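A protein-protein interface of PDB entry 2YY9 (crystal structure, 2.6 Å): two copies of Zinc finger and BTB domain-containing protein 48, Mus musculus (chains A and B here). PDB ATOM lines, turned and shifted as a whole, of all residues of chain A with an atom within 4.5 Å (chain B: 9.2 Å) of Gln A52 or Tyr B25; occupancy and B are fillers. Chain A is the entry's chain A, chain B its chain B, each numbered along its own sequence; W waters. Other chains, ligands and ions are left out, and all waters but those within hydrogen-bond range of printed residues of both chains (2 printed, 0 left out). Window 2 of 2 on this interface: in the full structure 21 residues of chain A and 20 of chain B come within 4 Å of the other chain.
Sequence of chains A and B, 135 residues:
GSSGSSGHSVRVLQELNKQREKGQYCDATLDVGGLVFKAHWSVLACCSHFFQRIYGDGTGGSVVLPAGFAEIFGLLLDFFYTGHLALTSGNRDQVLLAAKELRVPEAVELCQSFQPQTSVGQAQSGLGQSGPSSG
O of Ala A45 lies within hydrogen-bond range of NE2 of Gln A52. The backbone carbonyl oxygen (O) of Ser A48 sits close to the side-chain amide nitrogen (NE2) of Gln A52 (3.5 Å). The backbone carbonyl oxygen (O) of Gln B19 lies within hydrogen-bond range of the backbone NH (N) of Gln B24 (3.0 Å). A ring nitrogen (NE2) of His B40 is in hydrogen-bond range of the side-chain amide oxygen (OE1) of Gln B19. OH of Tyr B81 lies within hydrogen-bond range of N of His B40, 2.8 Å away.
Gln A52 touches one residue of chain B. Of chain A, only Ser A42, Ala A45, Gln A52 and Tyr A55 come within 4 Å of Tyr B25. Tyr A55 touches just one residue of chain B: Tyr B25. Printed residues of chain B within 4 Å of Ala A45: Gln B19 (3.8 Å) and Tyr B25 (3.4 Å). Printed residues of chain A within 4 Å of Leu B16: Ser A42 (3.4 Å). Gly B23 touches none of the printed residues of chain A. His A49 touches none of the printed residues of chain B. The nearest printed residue of chain A that does not touch Tyr B25 is Phe A51 (4.9 Å). The nearest printed residue of chain B that does not touch Ser A42 is Ser B42 (4.3 Å).
Among the printed residues, pairs that only touch across the chains: Tyr A55 with Tyr B25, Gln A52 with Tyr B25, Ser A42 with Leu B16, Ser A42 with His B40, Ala A45 with Tyr B25, Ala A45 with Gln B19 and Ser A42 with Tyr B25.
The backbone carbonyl oxygen (O) of Ser A42 lies within hydrogen-bond range of the side-chain amide nitrogen (NE2) of Gln B19.
Hydrophobic or aromatic side chains of chain B that line the printed part of chain A: Leu B16, Tyr B25 and His B40. Of the 10 printed residues of chain A, 4 touch a printed residue of chain B. Hydrophobic or aromatic side chains of chain A that line the printed part of chain B: Ala A45 and Tyr A55. Along chain A the printed residues that touch a printed residue of chain B span positions 42 to 55. Among the printed residues, 8 pairs touch across the chains.
Water W2 bridges OG of Ser B42 and OG of Ser A42. Water W1 lies within hydrogen-bond range of OE2 of Glu B15, NE2 of Gln B19 and O of Ala A45.
Position printed for both chains: 42. Of the 8 pairs that touch across the chains among the printed residues, none has its exchanged pair printed and touching as well.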
ATOM      1  N   SER A  42       0.056 -13.648  14.019  1.00  0.00           N
ATOM      2  CA  SER A  42      -1.048 -14.085  13.170  1.00  0.00           C
ATOM      3  C   SER A  42      -0.976 -13.537  11.745  1.00  0.00           C
ATOM      4  O   SER A  42      -1.285 -14.253  10.800  1.00  0.00           O
ATOM      5  CB  SER A  42      -2.397 -13.708  13.810  1.00  0.00           C
ATOM      6  OG  SER A  42      -2.541 -12.308  13.991  1.00  0.00           O
ATOM      7  N   ALA A  45       2.015 -15.122   9.949  1.00  0.00           N
ATOM      8  CA  ALA A  45       1.749 -16.499   9.546  1.00  0.00           C
ATOM      9  C   ALA A  45       0.904 -16.570   8.276  1.00  0.00           C
ATOM     10  O   ALA A  45       0.955 -17.559   7.549  1.00  0.00           O
ATOM     11  CB  ALA A  45       1.059 -17.260  10.673  1.00  0.00           C
ATOM     12  N   SER A  48       3.797 -15.839   5.462  1.00  0.00           N
ATOM     13  CA  SER A  48       5.114 -16.453   5.542  1.00  0.00           C
ATOM     14  C   SER A  48       5.192 -17.850   6.150  1.00  0.00           C
ATOM     15  O   SER A  48       4.750 -18.078   7.271  1.00  0.00           O
ATOM     16  CB  SER A  48       6.037 -15.519   6.313  1.00  0.00           C
ATOM     17  OG  SER A  48       7.206 -16.190   6.728  1.00  0.00           O
ATOM     18  N   HIS A  49       5.771 -18.784   5.407  1.00  0.00           N
ATOM     19  CA  HIS A  49       5.920 -20.144   5.908  1.00  0.00           C
ATOM     20  C   HIS A  49       7.038 -20.175   6.934  1.00  0.00           C
ATOM     21  O   HIS A  49       7.029 -21.005   7.835  1.00  0.00           O
ATOM     22  CB  HIS A  49       6.219 -21.124   4.767  1.00  0.00           C
ATOM     23  CG  HIS A  49       5.091 -21.274   3.795  1.00  0.00           C
ATOM     24  ND1 HIS A  49       3.829 -21.676   4.176  1.00  0.00           N
ATOM     25  CD2 HIS A  49       5.024 -21.045   2.461  1.00  0.00           C
ATOM     26  CE1 HIS A  49       3.033 -21.684   3.121  1.00  0.00           C
ATOM     27  NE2 HIS A  49       3.735 -21.305   2.068  1.00  0.00           N
ATOM     28  N   PHE A  50       7.994 -19.256   6.799  1.00  0.00           N
ATOM     29  CA  PHE A  50       9.116 -19.169   7.732  1.00  0.00           C
ATOM     30  C   PHE A  50       8.615 -18.760   9.108  1.00  0.00           C
ATOM     31  O   PHE A  50       9.042 -19.315  10.118  1.00  0.00           O
ATOM     32  CB  PHE A  50      10.164 -18.167   7.224  1.00  0.00           C
ATOM     33  CG  PHE A  50      11.165 -17.727   8.271  1.00  0.00           C
ATOM     34  CD1 PHE A  50      10.887 -16.647   9.118  1.00  0.00           C
ATOM     35  CD2 PHE A  50      12.398 -18.374   8.397  1.00  0.00           C
ATOM     36  CE1 PHE A  50      11.817 -16.216  10.072  1.00  0.00           C
ATOM     37  CE2 PHE A  50      13.344 -17.950   9.351  1.00  0.00           C
ATOM     38  CZ  PHE A  50      13.049 -16.868  10.190  1.00  0.00           C
ATOM     39  N   PHE A  51       7.703 -17.793   9.156  1.00  0.00           N
ATOM     40  CA  PHE A  51       7.172 -17.354  10.439  1.00  0.00           C
ATOM     41  C   PHE A  51       6.211 -18.381  11.022  1.00  0.00           C
ATOM     42  O   PHE A  51       6.055 -18.491  12.234  1.00  0.00           O
ATOM     43  CB  PHE A  51       6.509 -15.989  10.296  1.00  0.00           C
ATOM     44  CG  PHE A  51       7.493 -14.864  10.126  1.00  0.00           C
ATOM     45  CD1 PHE A  51       7.552 -14.137   8.933  1.00  0.00           C
ATOM     46  CD2 PHE A  51       8.375 -14.544  11.151  1.00  0.00           C
ATOM     47  CE1 PHE A  51       8.478 -13.106   8.765  1.00  0.00           C
ATOM     48  CE2 PHE A  51       9.300 -13.520  10.996  1.00  0.00           C
ATOM     49  CZ  PHE A  51       9.351 -12.794   9.791  1.00  0.00           C
ATOM     50  N   GLN A  52       5.571 -19.150  10.160  1.00  0.00           N
ATOM     51  CA  GLN A  52       4.678 -20.179  10.650  1.00  0.00           C
ATOM     52  C   GLN A  52       5.517 -21.199  11.420  1.00  0.00           C
ATOM     53  O   GLN A  52       5.159 -21.624  12.516  1.00  0.00           O
ATOM     54  CB  GLN A  52       3.974 -20.872   9.481  1.00  0.00           C
ATOM     55  CG  GLN A  52       2.783 -20.120   8.941  1.00  0.00           C
ATOM     56  CD  GLN A  52       2.285 -20.706   7.644  1.00  0.00           C
ATOM     57  OE1 GLN A  52       2.311 -21.918   7.454  1.00  0.00           O
ATOM     58  NE2 GLN A  52       1.819 -19.853   6.745  1.00  0.00           N
ATOM     59  N   ARG A  53       6.655 -21.559  10.841  1.00  0.00           N
ATOM     60  CA  ARG A  53       7.543 -22.553  11.422  1.00  0.00           C
ATOM     61  C   ARG A  53       8.278 -22.199  12.708  1.00  0.00           C
ATOM     62  O   ARG A  53       8.417 -23.050  13.582  1.00  0.00           O
ATOM     63  CB  ARG A  53       8.547 -23.020  10.359  1.00  0.00           C
ATOM     64  CG  ARG A  53       7.883 -23.836   9.247  1.00  0.00           C
ATOM     65  CD  ARG A  53       8.849 -24.215   8.132  1.00  0.00           C
ATOM     66  NE  ARG A  53       8.211 -25.049   7.109  1.00  0.00           N
ATOM     67  CZ  ARG A  53       7.734 -26.275   7.326  1.00  0.00           C
ATOM     68  NH1 ARG A  53       7.815 -26.823   8.534  1.00  0.00           N
ATOM     69  NH2 ARG A  53       7.178 -26.961   6.329  1.00  0.00           N
ATOM     70  N   ILE A  54       8.739 -20.962  12.844  1.00  0.00           N
ATOM     71  CA  ILE A  54       9.474 -20.596  14.045  1.00  0.00           C
ATOM     72  C   ILE A  54       8.601 -20.046  15.157  1.00  0.00           C
ATOM     73  O   ILE A  54       9.090 -19.381  16.065  1.00  0.00           O
ATOM     74  CB  ILE A  54      10.580 -19.567  13.743  1.00  0.00           C
ATOM     75  CG1 ILE A  54       9.953 -18.217  13.379  1.00  0.00           C
ATOM     76  CG2 ILE A  54      11.487 -20.100  12.624  1.00  0.00           C
ATOM     77  CD1 ILE A  54      10.919 -17.068  13.461  1.00  0.00           C
ATOM     78  N   TYR A  55       7.308 -20.321  15.083  1.00  0.00           N
ATOM     79  CA  TYR A  55       6.370 -19.859  16.104  1.00  0.00           C
ATOM     80  C   TYR A  55       6.135 -20.972  17.131  1.00  0.00           C
ATOM     81  O   TYR A  55       5.732 -22.078  16.777  1.00  0.00           O
ATOM     82  CB  TYR A  55       5.055 -19.440  15.431  1.00  0.00           C
ATOM     83  CG  TYR A  55       3.917 -19.120  16.373  1.00  0.00           C
ATOM     84  CD1 TYR A  55       3.099 -20.131  16.880  1.00  0.00           C
ATOM     85  CD2 TYR A  55       3.636 -17.806  16.732  1.00  0.00           C
ATOM     86  CE1 TYR A  55       2.022 -19.838  17.717  1.00  0.00           C
ATOM     87  CE2 TYR A  55       2.567 -17.501  17.567  1.00  0.00           C
ATOM     88  CZ  TYR A  55       1.763 -18.518  18.054  1.00  0.00           C
ATOM     89  OH  TYR A  55       0.688 -18.211  18.856  1.00  0.00           O
ATOM     90  N   GLU B  15      -7.787 -15.744   6.281  1.00  0.00           N
ATOM     91  CA  GLU B  15      -6.773 -16.650   6.799  1.00  0.00           C
ATOM     92  C   GLU B  15      -6.754 -16.562   8.321  1.00  0.00           C
ATOM     93  O   GLU B  15      -6.596 -17.567   9.007  1.00  0.00           O
ATOM     94  CB  GLU B  15      -5.406 -16.292   6.217  1.00  0.00           C
ATOM     95  CG  GLU B  15      -4.316 -17.317   6.493  1.00  0.00           C
ATOM     96  CD  GLU B  15      -4.717 -18.739   6.096  1.00  0.00           C
ATOM     97  OE1 GLU B  15      -5.218 -18.940   4.958  1.00  0.00           O
ATOM     98  OE2 GLU B  15      -4.519 -19.657   6.927  1.00  0.00           O
ATOM     99  N   LEU B  16      -6.916 -15.351   8.846  1.00  0.00           N
ATOM    100  CA  LEU B  16      -6.954 -15.150  10.288  1.00  0.00           C
ATOM    101  C   LEU B  16      -8.235 -15.819  10.780  1.00  0.00           C
ATOM    102  O   LEU B  16      -8.262 -16.394  11.859  1.00  0.00           O
ATOM    103  CB  LEU B  16      -6.975 -13.655  10.636  1.00  0.00           C
ATOM    104  CG  LEU B  16      -5.711 -12.825  10.366  1.00  0.00           C
ATOM    105  CD1 LEU B  16      -6.017 -11.335  10.568  1.00  0.00           C
ATOM    106  CD2 LEU B  16      -4.580 -13.267  11.289  1.00  0.00           C
ATOM    107  N   LYS B  18      -9.700 -18.416   9.409  1.00  0.00           N
ATOM    108  CA  LYS B  18      -9.376 -19.830   9.351  1.00  0.00           C
ATOM    109  C   LYS B  18      -8.535 -20.173  10.584  1.00  0.00           C
ATOM    110  O   LYS B  18      -8.810 -21.139  11.295  1.00  0.00           O
ATOM    111  CB  LYS B  18      -8.596 -20.117   8.072  1.00  0.00           C
ATOM    112  CG  LYS B  18      -8.402 -21.585   7.781  1.00  0.00           C
ATOM    113  CD  LYS B  18      -7.870 -21.797   6.371  1.00  0.00           C
ATOM    114  CE  LYS B  18      -7.645 -23.279   6.083  1.00  0.00           C
ATOM    115  NZ  LYS B  18      -7.022 -23.491   4.741  1.00  0.00           N
ATOM    116  N   GLN B  19      -7.516 -19.363  10.840  1.00  0.00           N
ATOM    117  CA  GLN B  19      -6.656 -19.564  11.994  1.00  0.00           C
ATOM    118  C   GLN B  19      -7.424 -19.758  13.310  1.00  0.00           C
ATOM    119  O   GLN B  19      -7.290 -20.800  13.966  1.00  0.00           O
ATOM    120  CB  GLN B  19      -5.710 -18.384  12.145  1.00  0.00           C
ATOM    121  CG  GLN B  19      -4.468 -18.469  11.317  1.00  0.00           C
ATOM    122  CD  GLN B  19      -3.591 -17.248  11.501  1.00  0.00           C
ATOM    123  OE1 GLN B  19      -3.691 -16.553  12.512  1.00  0.00           O
ATOM    124  NE2 GLN B  19      -2.719 -16.985  10.531  1.00  0.00           N
ATOM    125  N   ARG B  20      -8.220 -18.759  13.692  1.00  0.00           N
ATOM    126  CA  ARG B  20      -8.974 -18.816  14.940  1.00  0.00           C
ATOM    127  C   ARG B  20      -9.984 -19.960  14.991  1.00  0.00           C
ATOM    128  O   ARG B  20     -10.378 -20.397  16.075  1.00  0.00           O
ATOM    129  CB  ARG B  20      -9.668 -17.473  15.217  1.00  0.00           C
ATOM    130  CG  ARG B  20     -10.730 -17.078  14.221  1.00  0.00           C
ATOM    131  CD  ARG B  20     -12.125 -17.173  14.812  1.00  0.00           C
ATOM    132  NE  ARG B  20     -13.137 -16.885  13.799  1.00  0.00           N
ATOM    133  CZ  ARG B  20     -14.448 -16.958  14.001  1.00  0.00           C
ATOM    134  NH1 ARG B  20     -14.920 -17.307  15.185  1.00  0.00           N
ATOM    135  NH2 ARG B  20     -15.287 -16.694  13.015  1.00  0.00           N
ATOM    136  N   GLU B  21     -10.392 -20.454  13.826  1.00  0.00           N
ATOM    137  CA  GLU B  21     -11.335 -21.569  13.779  1.00  0.00           C
ATOM    138  C   GLU B  21     -10.572 -22.865  14.053  1.00  0.00           C
ATOM    139  O   GLU B  21     -11.123 -23.956  13.955  1.00  0.00           O
ATOM    140  CB  GLU B  21     -12.010 -21.650  12.406  1.00  0.00           C
ATOM    141  CG  GLU B  21     -12.802 -20.405  12.016  1.00  0.00           C
ATOM    142  CD  GLU B  21     -14.140 -20.303  12.722  1.00  0.00           C
ATOM    143  OE1 GLU B  21     -14.170 -20.406  13.970  1.00  0.00           O
ATOM    144  OE2 GLU B  21     -15.160 -20.112  12.022  1.00  0.00           O
ATOM    145  N   LYS B  22      -9.292 -22.727  14.387  1.00  0.00           N
ATOM    146  CA  LYS B  22      -8.431 -23.868  14.680  1.00  0.00           C
ATOM    147  C   LYS B  22      -7.557 -23.534  15.885  1.00  0.00           C
ATOM    148  O   LYS B  22      -6.738 -24.344  16.320  1.00  0.00           O
ATOM    149  CB  LYS B  22      -7.541 -24.190  13.477  1.00  0.00           C
ATOM    150  CG  LYS B  22      -8.291 -24.637  12.230  1.00  0.00           C
ATOM    151  CD  LYS B  22      -7.333 -25.218  11.184  1.00  0.00           C
ATOM    152  CE  LYS B  22      -8.091 -25.899  10.034  1.00  0.00           C
ATOM    153  NZ  LYS B  22      -7.196 -26.606   9.056  1.00  0.00           N
ATOM    154  N   GLY B  23      -7.734 -22.326  16.411  1.00  0.00           N
ATOM    155  CA  GLY B  23      -6.958 -21.897  17.560  1.00  0.00           C
ATOM    156  C   GLY B  23      -5.496 -21.614  17.273  1.00  0.00           C
ATOM    157  O   GLY B  23      -4.676 -21.630  18.182  1.00  0.00           O
ATOM    158  N   GLN B  24      -5.161 -21.333  16.020  1.00  0.00           N
ATOM    159  CA  GLN B  24      -3.773 -21.063  15.657  1.00  0.00           C
ATOM    160  C   GLN B  24      -3.394 -19.592  15.802  1.00  0.00           C
ATOM    161  O   GLN B  24      -4.149 -18.701  15.421  1.00  0.00           O
ATOM    162  CB  GLN B  24      -3.512 -21.523  14.228  1.00  0.00           C
ATOM    163  CG  GLN B  24      -3.975 -22.937  13.948  1.00  0.00           C
ATOM    164  CD  GLN B  24      -3.701 -23.362  12.521  1.00  0.00           C
ATOM    165  OE1 GLN B  24      -3.945 -22.606  11.575  1.00  0.00           O
ATOM    166  NE2 GLN B  24      -3.202 -24.584  12.354  1.00  0.00           N
ATOM    167  N   TYR B  25      -2.213 -19.358  16.367  1.00  0.00           N
ATOM    168  CA  TYR B  25      -1.680 -18.012  16.591  1.00  0.00           C
ATOM    169  C   TYR B  25      -2.666 -17.116  17.335  1.00  0.00           C
ATOM    170  O   TYR B  25      -2.576 -15.894  17.259  1.00  0.00           O
ATOM    171  CB  TYR B  25      -1.300 -17.365  15.253  1.00  0.00           C
ATOM    172  CG  TYR B  25      -0.527 -18.292  14.340  1.00  0.00           C
ATOM    173  CD1 TYR B  25       0.802 -18.632  14.609  1.00  0.00           C
ATOM    174  CD2 TYR B  25      -1.145 -18.878  13.240  1.00  0.00           C
ATOM    175  CE1 TYR B  25       1.490 -19.537  13.806  1.00  0.00           C
ATOM    176  CE2 TYR B  25      -0.472 -19.782  12.431  1.00  0.00           C
ATOM    177  CZ  TYR B  25       0.844 -20.113  12.715  1.00  0.00           C
ATOM    178  OH  TYR B  25       1.495 -21.027  11.903  1.00  0.00           O
ATOM    179  N   CYS B  26      -3.601 -17.726  18.059  1.00  0.00           N
ATOM    180  CA  CYS B  26      -4.597 -16.979  18.813  1.00  0.00           C
ATOM    181  C   CYS B  26      -4.114 -16.685  20.220  1.00  0.00           C
ATOM    182  O   CYS B  26      -3.731 -17.593  20.942  1.00  0.00           O
ATOM    183  CB  CYS B  26      -5.903 -17.763  18.887  1.00  0.00           C
ATOM    184  SG  CYS B  26      -6.732 -17.966  17.311  1.00  0.00           S
ATOM    185  N   ASP B  27      -4.142 -15.416  20.613  1.00  0.00           N
ATOM    186  CA  ASP B  27      -3.699 -15.031  21.947  1.00  0.00           C
ATOM    187  C   ASP B  27      -4.863 -14.764  22.901  1.00  0.00           C
ATOM    188  O   ASP B  27      -4.656 -14.391  24.050  1.00  0.00           O
ATOM    189  CB  ASP B  27      -2.781 -13.798  21.876  1.00  0.00           C
ATOM    190  CG  ASP B  27      -3.321 -12.699  20.954  1.00  0.00           C
ATOM    191  OD1 ASP B  27      -4.490 -12.778  20.513  1.00  0.00           O
ATOM    192  OD2 ASP B  27      -2.566 -11.745  20.674  1.00  0.00           O
ATOM    193  N   ALA B  28      -6.087 -14.966  22.429  1.00  0.00           N
ATOM    194  CA  ALA B  28      -7.252 -14.741  23.271  1.00  0.00           C
ATOM    195  C   ALA B  28      -8.155 -15.968  23.374  1.00  0.00           C
ATOM    196  O   ALA B  28      -8.393 -16.671  22.391  1.00  0.00           O
ATOM    197  CB  ALA B  28      -8.050 -13.549  22.751  1.00  0.00           C
ATOM    198  N   LYS B  38     -11.576 -19.158  20.452  1.00  0.00           N
ATOM    199  CA  LYS B  38     -10.208 -18.677  20.360  1.00  0.00           C
ATOM    200  C   LYS B  38     -10.241 -17.496  19.387  1.00  0.00           C
ATOM    201  O   LYS B  38     -10.972 -17.515  18.400  1.00  0.00           O
ATOM    202  CB  LYS B  38      -9.289 -19.776  19.827  1.00  0.00           C
ATOM    203  CG  LYS B  38      -9.165 -20.973  20.742  1.00  0.00           C
ATOM    204  CD  LYS B  38      -8.415 -20.635  22.023  1.00  0.00           C
ATOM    205  CE  LYS B  38      -8.477 -21.798  23.006  1.00  0.00           C
ATOM    206  NZ  LYS B  38      -8.180 -23.094  22.322  1.00  0.00           N
ATOM    207  N   ALA B  39      -9.464 -16.460  19.667  1.00  0.00           N
ATOM    208  CA  ALA B  39      -9.444 -15.304  18.785  1.00  0.00           C
ATOM    209  C   ALA B  39      -8.132 -14.558  18.907  1.00  0.00           C
ATOM    210  O   ALA B  39      -7.242 -14.979  19.632  1.00  0.00           O
ATOM    211  CB  ALA B  39     -10.611 -14.375  19.109  1.00  0.00           C
ATOM    212  N   HIS B  40      -8.018 -13.461  18.168  1.00  0.00           N
ATOM    213  CA  HIS B  40      -6.832 -12.621  18.183  1.00  0.00           C
ATOM    214  C   HIS B  40      -7.221 -11.308  18.848  1.00  0.00           C
ATOM    215  O   HIS B  40      -8.193 -10.667  18.439  1.00  0.00           O
ATOM    216  CB  HIS B  40      -6.349 -12.320  16.758  1.00  0.00           C
ATOM    217  CG  HIS B  40      -6.037 -13.537  15.943  1.00  0.00           C
ATOM    218  ND1 HIS B  40      -6.903 -14.042  14.999  1.00  0.00           N
ATOM    219  CD2 HIS B  40      -4.949 -14.343  15.926  1.00  0.00           C
ATOM    220  CE1 HIS B  40      -6.363 -15.107  14.435  1.00  0.00           C
ATOM    221  NE2 HIS B  40      -5.177 -15.311  14.980  1.00  0.00           N
ATOM    222  N   TRP B  41      -6.470 -10.911  19.870  1.00  0.00           N
ATOM    223  CA  TRP B  41      -6.760  -9.669  20.560  1.00  0.00           C
ATOM    224  C   TRP B  41      -6.700  -8.525  19.566  1.00  0.00           C
ATOM    225  O   TRP B  41      -7.550  -7.644  19.575  1.00  0.00           O
ATOM    226  CB  TRP B  41      -5.759  -9.432  21.693  1.00  0.00           C
ATOM    227  CG  TRP B  41      -6.052 -10.225  22.939  1.00  0.00           C
ATOM    228  CD1 TRP B  41      -5.344 -11.284  23.424  1.00  0.00           C
ATOM    229  CD2 TRP B  41      -7.135 -10.018  23.855  1.00  0.00           C
ATOM    230  NE1 TRP B  41      -5.915 -11.748  24.582  1.00  0.00           N
ATOM    231  CE2 TRP B  41      -7.017 -10.992  24.869  1.00  0.00           C
ATOM    232  CE3 TRP B  41      -8.196  -9.102  23.916  1.00  0.00           C
ATOM    233  CZ2 TRP B  41      -7.919 -11.079  25.935  1.00  0.00           C
ATOM    234  CZ3 TRP B  41      -9.095  -9.189  24.976  1.00  0.00           C
ATOM    235  CH2 TRP B  41      -8.950 -10.172  25.971  1.00  0.00           C
ATOM    236  N   SER B  42      -5.690  -8.553  18.706  1.00  0.00           N
ATOM    237  CA  SER B  42      -5.496  -7.521  17.698  1.00  0.00           C
ATOM    238  C   SER B  42      -6.767  -7.273  16.897  1.00  0.00           C
ATOM    239  O   SER B  42      -7.129  -6.123  16.632  1.00  0.00           O
ATOM    240  CB  SER B  42      -4.353  -7.918  16.758  1.00  0.00           C
ATOM    241  OG  SER B  42      -4.571  -9.183  16.154  1.00  0.00           O
ATOM    242  N   VAL B  43      -7.446  -8.351  16.511  1.00  0.00           N
ATOM    243  CA  VAL B  43      -8.683  -8.237  15.745  1.00  0.00           C
ATOM    244  C   VAL B  43      -9.843  -7.875  16.676  1.00  0.00           C
ATOM    245  O   VAL B  43     -10.730  -7.114  16.299  1.00  0.00           O
ATOM    246  CB  VAL B  43      -8.994  -9.561  15.002  1.00  0.00           C
ATOM    247  CG1 VAL B  43     -10.371  -9.500  14.360  1.00  0.00           C
ATOM    248  CG2 VAL B  43      -7.941  -9.820  13.950  1.00  0.00           C
ATOM    249  N   TYR B  81     -14.470 -11.329  11.977  1.00  0.00           N
ATOM    250  CA  TYR B  81     -13.583 -11.867  10.965  1.00  0.00           C
ATOM    251  C   TYR B  81     -14.099 -11.917   9.527  1.00  0.00           C
ATOM    252  O   TYR B  81     -13.348 -12.273   8.621  1.00  0.00           O
ATOM    253  CB  TYR B  81     -13.120 -13.265  11.388  1.00  0.00           C
ATOM    254  CG  TYR B  81     -12.172 -13.260  12.571  1.00  0.00           C
ATOM    255  CD1 TYR B  81     -12.649 -13.171  13.878  1.00  0.00           C
ATOM    256  CD2 TYR B  81     -10.792 -13.332  12.378  1.00  0.00           C
ATOM    257  CE1 TYR B  81     -11.770 -13.157  14.963  1.00  0.00           C
ATOM    258  CE2 TYR B  81      -9.908 -13.317  13.448  1.00  0.00           C
ATOM    259  CZ  TYR B  81     -10.400 -13.230  14.735  1.00  0.00           C
ATOM    260  OH  TYR B  81      -9.519 -13.218  15.790  1.00  0.00           O
HETATM  261  O   HOH W   1      -1.937 -19.032   8.387  1.00  0.00           O
HETATM  262  O   HOH W   2      -2.627 -10.908  16.754  1.00  0.00           O
